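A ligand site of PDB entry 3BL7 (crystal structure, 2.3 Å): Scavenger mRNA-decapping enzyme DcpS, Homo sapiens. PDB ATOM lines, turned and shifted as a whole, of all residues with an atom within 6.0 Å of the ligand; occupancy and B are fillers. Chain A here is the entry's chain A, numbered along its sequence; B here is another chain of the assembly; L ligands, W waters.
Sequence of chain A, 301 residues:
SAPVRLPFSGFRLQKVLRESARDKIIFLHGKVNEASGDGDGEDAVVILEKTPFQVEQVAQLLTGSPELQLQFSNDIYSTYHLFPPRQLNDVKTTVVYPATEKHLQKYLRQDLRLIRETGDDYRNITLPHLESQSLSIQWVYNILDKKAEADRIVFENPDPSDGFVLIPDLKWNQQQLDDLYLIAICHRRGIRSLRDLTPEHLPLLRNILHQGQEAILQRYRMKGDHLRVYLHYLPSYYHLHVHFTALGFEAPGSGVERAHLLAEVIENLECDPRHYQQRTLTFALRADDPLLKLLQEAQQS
O of Pro 168 is in hydrogen-bond range of N4 of the ligand, at 2.7 Å.
OE1 of Glu 149 is in hydrogen-bond range of N5 of the ligand, at 2.7 Å.
The side-chain carboxylate (OD2) of Asp 169 lies within hydrogen-bond range of a nitrogen (N2) of the ligand (3.1 Å).
N3 of the ligand lies within hydrogen-bond range of N of Leu 170 (3.2 Å).
O of Pro 168 is in hydrogen-bond range of NH1 of Arg 152 (3.3 Å).
OE2 of Glu 149 lies within salt-bridge range of NH1 of Arg 152 (2.9 Å).
The side-chain carboxylate of Glu 149 lies within hydrogen-bond range of the side-chain amide nitrogen of Asn 74 of chain B (2.9 Å).
OG of Ser 236 sits at hydrogen-bond distance from NH2 of Arg 258.
The side-chain carboxylate (OD1) of Asp 169 sits at hydrogen-bond distance from the backbone NH (N) of Lys 171 (2.9 Å).
O of Trp 139 lies within hydrogen-bond range of ND2 of Asn 74 of chain B, at 3.1 Å.
The side-chain hydroxyl of Tyr 107 lies within hydrogen-bond range of the side-chain amino group of Lys 106 (3.0 Å).
The backbone NH of Ile 183 lies within hydrogen-bond range of the backbone carbonyl oxygen of Ile 167, at 2.8 Å.
The side-chain hydroxyl (OG) of Ser 236 lies close to a fluorine (F1) of the ligand.
Lys 106 touches the ligand.
CD2 of Tyr 107 touches C3 of the ligand, 3.4 Å away.
Trp 139 touches the ligand.
Ile 143 touches the ligand (CD1 to N5, 3.9 Å).
NH1 of Arg 152 touches N4 of the ligand, at 3.8 Å.
Ile 167 touches the ligand (CG2 to N4, 3.9 Å).
CD1 of Ile 183 touches N3 of the ligand, 3.6 Å away.
Phe 72 of chain B touches the ligand.
Asn 74 of chain B touches the ligand.
CD1 of Tyr 77 of chain B touches C21 of the ligand, at 3.4 Å.
Hydrophobic or aromatic side chains within 4 Å of the ligand: Tyr 107, Trp 139, Ile 143, Ile 167, Leu 170, Ile 183, Phe 72 of chain B and Tyr 77 of chain B.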
ATOM      1  N   ARG A  18     -26.702  16.203   3.979  1.00  0.00           N
ATOM      2  CA  ARG A  18     -25.603  16.309   3.031  1.00  0.00           C
ATOM      3  C   ARG A  18     -25.204  14.903   2.531  1.00  0.00           C
ATOM      4  O   ARG A  18     -25.420  13.904   3.220  1.00  0.00           O
ATOM      5  CB  ARG A  18     -24.428  16.999   3.705  1.00  0.00           C
ATOM      6  CG  ARG A  18     -23.263  17.333   2.796  1.00  0.00           C
ATOM      7  CD  ARG A  18     -22.060  17.775   3.595  1.00  0.00           C
ATOM      8  NE  ARG A  18     -22.284  19.076   4.219  1.00  0.00           N
ATOM      9  CZ  ARG A  18     -21.418  19.689   5.026  1.00  0.00           C
ATOM     10  NH1 ARG A  18     -20.228  19.136   5.323  1.00  0.00           N
ATOM     11  NH2 ARG A  18     -21.744  20.874   5.547  1.00  0.00           N
ATOM     12  N   PHE A  27     -24.743  12.530   5.806  1.00  0.00           N
ATOM     13  CA  PHE A  27     -25.240  13.201   7.010  1.00  0.00           C
ATOM     14  C   PHE A  27     -26.760  13.109   7.009  1.00  0.00           C
ATOM     15  O   PHE A  27     -27.406  13.643   6.105  1.00  0.00           O
ATOM     16  CB  PHE A  27     -24.834  14.685   7.024  1.00  0.00           C
ATOM     17  CG  PHE A  27     -23.338  14.928   7.022  1.00  0.00           C
ATOM     18  CD1 PHE A  27     -22.575  14.652   5.883  1.00  0.00           C
ATOM     19  CD2 PHE A  27     -22.703  15.419   8.140  1.00  0.00           C
ATOM     20  CE1 PHE A  27     -21.217  14.851   5.880  1.00  0.00           C
ATOM     21  CE2 PHE A  27     -21.336  15.632   8.151  1.00  0.00           C
ATOM     22  CZ  PHE A  27     -20.590  15.344   7.020  1.00  0.00           C
ATOM     23  N   LYS A 106     -26.054  23.442  10.472  1.00  0.00           N
ATOM     24  CA  LYS A 106     -24.600  23.217  10.405  1.00  0.00           C
ATOM     25  C   LYS A 106     -24.166  22.166   9.370  1.00  0.00           C
ATOM     26  O   LYS A 106     -23.319  22.420   8.530  1.00  0.00           O
ATOM     27  CB  LYS A 106     -24.120  22.834  11.825  1.00  0.00           C
ATOM     28  CG  LYS A 106     -22.666  22.396  12.022  1.00  0.00           C
ATOM     29  CD  LYS A 106     -22.237  22.652  13.495  1.00  0.00           C
ATOM     30  CE  LYS A 106     -21.052  21.787  13.962  1.00  0.00           C
ATOM     31  NZ  LYS A 106     -21.461  20.598  14.794  1.00  0.00           N
ATOM     32  N   TYR A 107     -24.769  20.985   9.436  1.00  0.00           N
ATOM     33  CA  TYR A 107     -24.405  19.843   8.570  1.00  0.00           C
ATOM     34  C   TYR A 107     -25.150  19.802   7.218  1.00  0.00           C
ATOM     35  O   TYR A 107     -25.058  18.816   6.479  1.00  0.00           O
ATOM     36  CB  TYR A 107     -24.643  18.522   9.329  1.00  0.00           C
ATOM     37  CG  TYR A 107     -23.752  18.341  10.533  1.00  0.00           C
ATOM     38  CD1 TYR A 107     -24.290  18.117  11.803  1.00  0.00           C
ATOM     39  CD2 TYR A 107     -22.374  18.382  10.402  1.00  0.00           C
ATOM     40  CE1 TYR A 107     -23.473  17.927  12.908  1.00  0.00           C
ATOM     41  CE2 TYR A 107     -21.539  18.205  11.499  1.00  0.00           C
ATOM     42  CZ  TYR A 107     -22.091  17.988  12.751  1.00  0.00           C
ATOM     43  OH  TYR A 107     -21.254  17.817  13.826  1.00  0.00           O
ATOM     44  N   TRP A 139     -18.233  19.543  25.435  1.00  0.00           N
ATOM     45  CA  TRP A 139     -17.349  18.441  25.072  1.00  0.00           C
ATOM     46  C   TRP A 139     -15.883  18.811  25.252  1.00  0.00           C
ATOM     47  O   TRP A 139     -15.071  17.953  25.585  1.00  0.00           O
ATOM     48  CB  TRP A 139     -17.644  17.930  23.658  1.00  0.00           C
ATOM     49  CG  TRP A 139     -17.192  18.763  22.491  1.00  0.00           C
ATOM     50  CD1 TRP A 139     -17.955  19.625  21.755  1.00  0.00           C
ATOM     51  CD2 TRP A 139     -15.900  18.751  21.866  1.00  0.00           C
ATOM     52  NE1 TRP A 139     -17.222  20.171  20.744  1.00  0.00           N
ATOM     53  CE2 TRP A 139     -15.951  19.653  20.789  1.00  0.00           C
ATOM     54  CE3 TRP A 139     -14.705  18.072  22.115  1.00  0.00           C
ATOM     55  CZ2 TRP A 139     -14.847  19.888  19.953  1.00  0.00           C
ATOM     56  CZ3 TRP A 139     -13.614  18.318  21.304  1.00  0.00           C
ATOM     57  CH2 TRP A 139     -13.698  19.222  20.232  1.00  0.00           C
ATOM     58  N   ILE A 143     -13.164  17.164  28.114  1.00  0.00           N
ATOM     59  CA  ILE A 143     -11.820  16.661  27.862  1.00  0.00           C
ATOM     60  C   ILE A 143     -10.817  17.306  28.814  1.00  0.00           C
ATOM     61  O   ILE A 143     -10.015  16.607  29.447  1.00  0.00           O
ATOM     62  CB  ILE A 143     -11.363  16.921  26.392  1.00  0.00           C
ATOM     63  CG1 ILE A 143     -12.181  16.071  25.413  1.00  0.00           C
ATOM     64  CG2 ILE A 143      -9.870  16.579  26.223  1.00  0.00           C
ATOM     65  CD1 ILE A 143     -12.078  16.520  23.978  1.00  0.00           C
ATOM     66  N   GLU A 149     -13.193  11.070  27.843  1.00  0.00           N
ATOM     67  CA  GLU A 149     -12.020  10.780  27.012  1.00  0.00           C
ATOM     68  C   GLU A 149     -10.704  10.910  27.763  1.00  0.00           C
ATOM     69  O   GLU A 149      -9.689  11.264  27.159  1.00  0.00           O
ATOM     70  CB  GLU A 149     -11.983  11.716  25.798  1.00  0.00           C
ATOM     71  CG  GLU A 149     -13.267  11.748  24.981  1.00  0.00           C
ATOM     72  CD  GLU A 149     -13.100  12.539  23.697  1.00  0.00           C
ATOM     73  OE1 GLU A 149     -13.827  13.513  23.484  1.00  0.00           O
ATOM     74  OE2 GLU A 149     -12.225  12.200  22.901  1.00  0.00           O
ATOM     75  N   ARG A 152      -7.872   8.610  26.567  1.00  0.00           N
ATOM     76  CA  ARG A 152      -7.471   8.762  25.169  1.00  0.00           C
ATOM     77  C   ARG A 152      -6.366   9.774  24.991  1.00  0.00           C
ATOM     78  O   ARG A 152      -5.796   9.891  23.910  1.00  0.00           O
ATOM     79  CB  ARG A 152      -8.655   9.169  24.300  1.00  0.00           C
ATOM     80  CG  ARG A 152      -9.815   8.229  24.388  1.00  0.00           C
ATOM     81  CD  ARG A 152     -10.990   8.782  23.620  1.00  0.00           C
ATOM     82  NE  ARG A 152     -10.892   8.399  22.219  1.00  0.00           N
ATOM     83  CZ  ARG A 152     -10.629   9.218  21.201  1.00  0.00           C
ATOM     84  NH1 ARG A 152     -10.465  10.515  21.380  1.00  0.00           N
ATOM     85  NH2 ARG A 152     -10.564   8.713  19.989  1.00  0.00           N
ATOM     86  N   ILE A 167      -5.018  15.150  21.920  1.00  0.00           N
ATOM     87  CA  ILE A 167      -5.948  14.015  21.895  1.00  0.00           C
ATOM     88  C   ILE A 167      -6.420  13.737  20.462  1.00  0.00           C
ATOM     89  O   ILE A 167      -6.530  14.669  19.665  1.00  0.00           O
ATOM     90  CB  ILE A 167      -7.160  14.271  22.828  1.00  0.00           C
ATOM     91  CG1 ILE A 167      -7.928  12.984  23.097  1.00  0.00           C
ATOM     92  CG2 ILE A 167      -8.075  15.382  22.265  1.00  0.00           C
ATOM     93  CD1 ILE A 167      -8.969  13.128  24.175  1.00  0.00           C
ATOM     94  N   PRO A 168      -6.656  12.450  20.114  1.00  0.00           N
ATOM     95  CA  PRO A 168      -7.189  12.187  18.771  1.00  0.00           C
ATOM     96  C   PRO A 168      -8.501  12.909  18.509  1.00  0.00           C
ATOM     97  O   PRO A 168      -9.363  12.966  19.384  1.00  0.00           O
ATOM     98  CB  PRO A 168      -7.404  10.657  18.766  1.00  0.00           C
ATOM     99  CG  PRO A 168      -6.426  10.139  19.762  1.00  0.00           C
ATOM    100  CD  PRO A 168      -6.383  11.192  20.846  1.00  0.00           C
ATOM    101  N   ASP A 169      -8.625  13.490  17.314  1.00  0.00           N
ATOM    102  CA  ASP A 169      -9.857  14.135  16.922  1.00  0.00           C
ATOM    103  C   ASP A 169     -10.901  13.058  16.619  1.00  0.00           C
ATOM    104  O   ASP A 169     -10.545  11.925  16.304  1.00  0.00           O
ATOM    105  CB  ASP A 169      -9.605  15.039  15.715  1.00  0.00           C
ATOM    106  CG  ASP A 169     -10.831  15.854  15.311  1.00  0.00           C
ATOM    107  OD1 ASP A 169     -11.671  15.354  14.539  1.00  0.00           O
ATOM    108  OD2 ASP A 169     -10.931  17.023  15.747  1.00  0.00           O
ATOM    109  N   LEU A 170     -12.176  13.430  16.740  1.00  0.00           N
ATOM    110  CA  LEU A 170     -13.351  12.553  16.471  1.00  0.00           C
ATOM    111  C   LEU A 170     -13.384  11.958  15.050  1.00  0.00           C
ATOM    112  O   LEU A 170     -13.790  10.808  14.862  1.00  0.00           O
ATOM    113  CB  LEU A 170     -14.645  13.350  16.738  1.00  0.00           C
ATOM    114  CG  LEU A 170     -16.028  12.782  16.394  1.00  0.00           C
ATOM    115  CD1 LEU A 170     -16.291  11.504  17.163  1.00  0.00           C
ATOM    116  CD2 LEU A 170     -17.098  13.774  16.680  1.00  0.00           C
ATOM    117  N   LYS A 171     -12.973  12.750  14.064  1.00  0.00           N
ATOM    118  CA  LYS A 171     -12.804  12.302  12.659  1.00  0.00           C
ATOM    119  C   LYS A 171     -11.953  11.024  12.519  1.00  0.00           C
ATOM    120  O   LYS A 171     -12.230  10.156  11.677  1.00  0.00           O
ATOM    121  CB  LYS A 171     -12.146  13.430  11.840  1.00  0.00           C
ATOM    122  CG  LYS A 171     -11.994  13.185  10.330  1.00  0.00           C
ATOM    123  CD  LYS A 171     -13.304  13.439   9.608  1.00  0.00           C
ATOM    124  CE  LYS A 171     -13.159  13.222   8.111  1.00  0.00           C
ATOM    125  NZ  LYS A 171     -14.243  13.886   7.339  1.00  0.00           N
ATOM    126  N   ILE A 183      -5.956  16.690  17.823  1.00  0.00           N
ATOM    127  CA  ILE A 183      -6.121  18.092  18.209  1.00  0.00           C
ATOM    128  C   ILE A 183      -5.395  18.362  19.540  1.00  0.00           C
ATOM    129  O   ILE A 183      -5.328  17.483  20.409  1.00  0.00           O
ATOM    130  CB  ILE A 183      -7.628  18.541  18.338  1.00  0.00           C
ATOM    131  CG1 ILE A 183      -8.443  17.508  19.121  1.00  0.00           C
ATOM    132  CG2 ILE A 183      -8.227  18.779  16.950  1.00  0.00           C
ATOM    133  CD1 ILE A 183      -9.864  17.948  19.403  1.00  0.00           C
ATOM    134  N   SER A 236     -14.489  25.885  13.736  1.00  0.00           N
ATOM    135  CA  SER A 236     -15.823  25.305  13.874  1.00  0.00           C
ATOM    136  C   SER A 236     -16.334  25.483  15.295  1.00  0.00           C
ATOM    137  O   SER A 236     -17.537  25.518  15.528  1.00  0.00           O
ATOM    138  CB  SER A 236     -15.805  23.822  13.526  1.00  0.00           C
ATOM    139  OG  SER A 236     -15.718  23.641  12.136  1.00  0.00           O
ATOM    140  N   TYR A 237     -15.410  25.603  16.243  1.00  0.00           N
ATOM    141  CA  TYR A 237     -15.753  25.898  17.621  1.00  0.00           C
ATOM    142  C   TYR A 237     -14.737  26.854  18.228  1.00  0.00           C
ATOM    143  O   TYR A 237     -13.556  26.833  17.877  1.00  0.00           O
ATOM    144  CB  TYR A 237     -15.879  24.615  18.443  1.00  0.00           C
ATOM    145  CG  TYR A 237     -14.752  23.633  18.258  1.00  0.00           C
ATOM    146  CD1 TYR A 237     -13.783  23.479  19.231  1.00  0.00           C
ATOM    147  CD2 TYR A 237     -14.660  22.861  17.103  1.00  0.00           C
ATOM    148  CE1 TYR A 237     -12.733  22.577  19.069  1.00  0.00           C
ATOM    149  CE2 TYR A 237     -13.622  21.951  16.942  1.00  0.00           C
ATOM    150  CZ  TYR A 237     -12.660  21.826  17.928  1.00  0.00           C
ATOM    151  OH  TYR A 237     -11.624  20.934  17.791  1.00  0.00           O
ATOM    152  N   ARG A 258      -8.405  28.317   4.713  1.00  0.00           N
ATOM    153  CA  ARG A 258      -8.787  28.060   6.101  1.00  0.00           C
ATOM    154  C   ARG A 258      -7.654  27.739   7.083  1.00  0.00           C
ATOM    155  O   ARG A 258      -7.750  28.070   8.259  1.00  0.00           O
ATOM    156  CB  ARG A 258      -9.838  26.944   6.154  1.00  0.00           C
ATOM    157  CG  ARG A 258     -10.571  26.920   7.496  1.00  0.00           C
ATOM    158  CD  ARG A 258     -11.771  26.027   7.488  1.00  0.00           C
ATOM    159  NE  ARG A 258     -12.429  26.081   8.781  1.00  0.00           N
ATOM    160  CZ  ARG A 258     -13.186  25.120   9.292  1.00  0.00           C
ATOM    161  NH1 ARG A 258     -13.381  23.988   8.629  1.00  0.00           N
ATOM    162  NH2 ARG A 258     -13.726  25.273  10.496  1.00  0.00           N
ATOM    163  N   PHE B  72     -15.854   5.874  21.264  1.00  0.00           N
ATOM    164  CA  PHE B  72     -15.919   6.691  22.494  1.00  0.00           C
ATOM    165  C   PHE B  72     -17.149   7.604  22.466  1.00  0.00           C
ATOM    166  O   PHE B  72     -17.690   7.898  21.388  1.00  0.00           O
ATOM    167  CB  PHE B  72     -14.641   7.538  22.693  1.00  0.00           C
ATOM    168  CG  PHE B  72     -14.529   8.722  21.758  1.00  0.00           C
ATOM    169  CD1 PHE B  72     -15.012   9.967  22.137  1.00  0.00           C
ATOM    170  CD2 PHE B  72     -13.927   8.600  20.521  1.00  0.00           C
ATOM    171  CE1 PHE B  72     -14.924  11.058  21.292  1.00  0.00           C
ATOM    172  CE2 PHE B  72     -13.823   9.692  19.659  1.00  0.00           C
ATOM    173  CZ  PHE B  72     -14.324  10.925  20.046  1.00  0.00           C
ATOM    174  N   ASN B  74     -18.718  11.486  24.356  1.00  0.00           N
ATOM    175  CA  ASN B  74     -18.486  12.716  25.093  1.00  0.00           C
ATOM    176  C   ASN B  74     -19.710  13.617  24.882  1.00  0.00           C
ATOM    177  O   ASN B  74     -19.959  14.065  23.750  1.00  0.00           O
ATOM    178  CB  ASN B  74     -17.217  13.403  24.591  1.00  0.00           C
ATOM    179  CG  ASN B  74     -16.792  14.609  25.449  1.00  0.00           C
ATOM    180  OD1 ASN B  74     -17.599  15.267  26.095  1.00  0.00           O
ATOM    181  ND2 ASN B  74     -15.487  14.885  25.442  1.00  0.00           N
ATOM    182  N   TYR B  77     -22.236  13.610  21.730  1.00  0.00           N
ATOM    183  CA  TYR B  77     -21.559  12.937  20.623  1.00  0.00           C
ATOM    184  C   TYR B  77     -21.115  11.516  20.960  1.00  0.00           C
ATOM    185  O   TYR B  77     -20.680  11.224  22.074  1.00  0.00           O
ATOM    186  CB  TYR B  77     -20.324  13.716  20.197  1.00  0.00           C
ATOM    187  CG  TYR B  77     -20.572  15.109  19.705  1.00  0.00           C
ATOM    188  CD1 TYR B  77     -20.557  16.179  20.600  1.00  0.00           C
ATOM    189  CD2 TYR B  77     -20.752  15.377  18.356  1.00  0.00           C
ATOM    190  CE1 TYR B  77     -20.758  17.469  20.159  1.00  0.00           C
ATOM    191  CE2 TYR B  77     -20.961  16.665  17.908  1.00  0.00           C
ATOM    192  CZ  TYR B  77     -20.951  17.717  18.816  1.00  0.00           C
ATOM    193  OH  TYR B  77     -21.134  19.004  18.385  1.00  0.00           O
HETATM  194  F1  LIG L   1     -18.367  22.360  11.755  1.00  0.00           F
HETATM  195  C1  LIG L   1     -18.601  21.309  10.951  1.00  0.00           C
HETATM  196  C2  LIG L   1     -19.651  21.368  10.040  1.00  0.00           C
HETATM  197  C3  LIG L   1     -19.894  20.286   9.197  1.00  0.00           C
HETATM  198  C4  LIG L   1     -19.101  19.140   9.251  1.00  0.00           C
HETATM  199  C5  LIG L   1     -18.034  19.036  10.146  1.00  0.00           C
HETATM  200  C6  LIG L   1     -17.752  20.083  11.036  1.00  0.00           C
HETATM  201  C7  LIG L   1     -16.572  19.961  11.984  1.00  0.00           C
HETATM  202  N1  LIG L   1     -16.832  19.751  13.419  1.00  0.00           N
HETATM  203  C8  LIG L   1     -18.083  20.118  14.078  1.00  0.00           C
HETATM  204  C9  LIG L   1     -17.972  19.755  15.567  1.00  0.00           C
HETATM  205  C10 LIG L   1     -17.553  18.298  15.794  1.00  0.00           C
HETATM  206  C11 LIG L   1     -16.277  17.989  14.996  1.00  0.00           C
HETATM  207  C12 LIG L   1     -15.736  19.181  14.218  1.00  0.00           C
HETATM  208  C13 LIG L   1     -17.442  17.966  17.302  1.00  0.00           C
HETATM  209  O1  LIG L   1     -16.191  17.455  17.820  1.00  0.00           O
HETATM  210  C14 LIG L   1     -16.136  16.650  18.948  1.00  0.00           C
HETATM  211  C15 LIG L   1     -14.864  15.996  19.377  1.00  0.00           C
HETATM  212  C16 LIG L   1     -13.568  16.151  18.653  1.00  0.00           C
HETATM  213  N2  LIG L   1     -13.453  16.907  17.545  1.00  0.00           N
HETATM  214  N3  LIG L   1     -12.498  15.512  19.128  1.00  0.00           N
HETATM  215  C17 LIG L   1     -12.560  14.737  20.247  1.00  0.00           C
HETATM  216  N4  LIG L   1     -11.420  14.140  20.660  1.00  0.00           N
HETATM  217  N5  LIG L   1     -13.694  14.557  20.973  1.00  0.00           N
HETATM  218  C18 LIG L   1     -14.847  15.137  20.595  1.00  0.00           C
HETATM  219  C19 LIG L   1     -16.005  14.956  21.317  1.00  0.00           C
HETATM  220  C20 LIG L   1     -17.180  15.584  20.885  1.00  0.00           C
HETATM  221  C21 LIG L   1     -17.249  16.397  19.739  1.00  0.00           C
HETATM  222  O   HOH W   1     -13.290  21.272  13.493  1.00  0.00           O
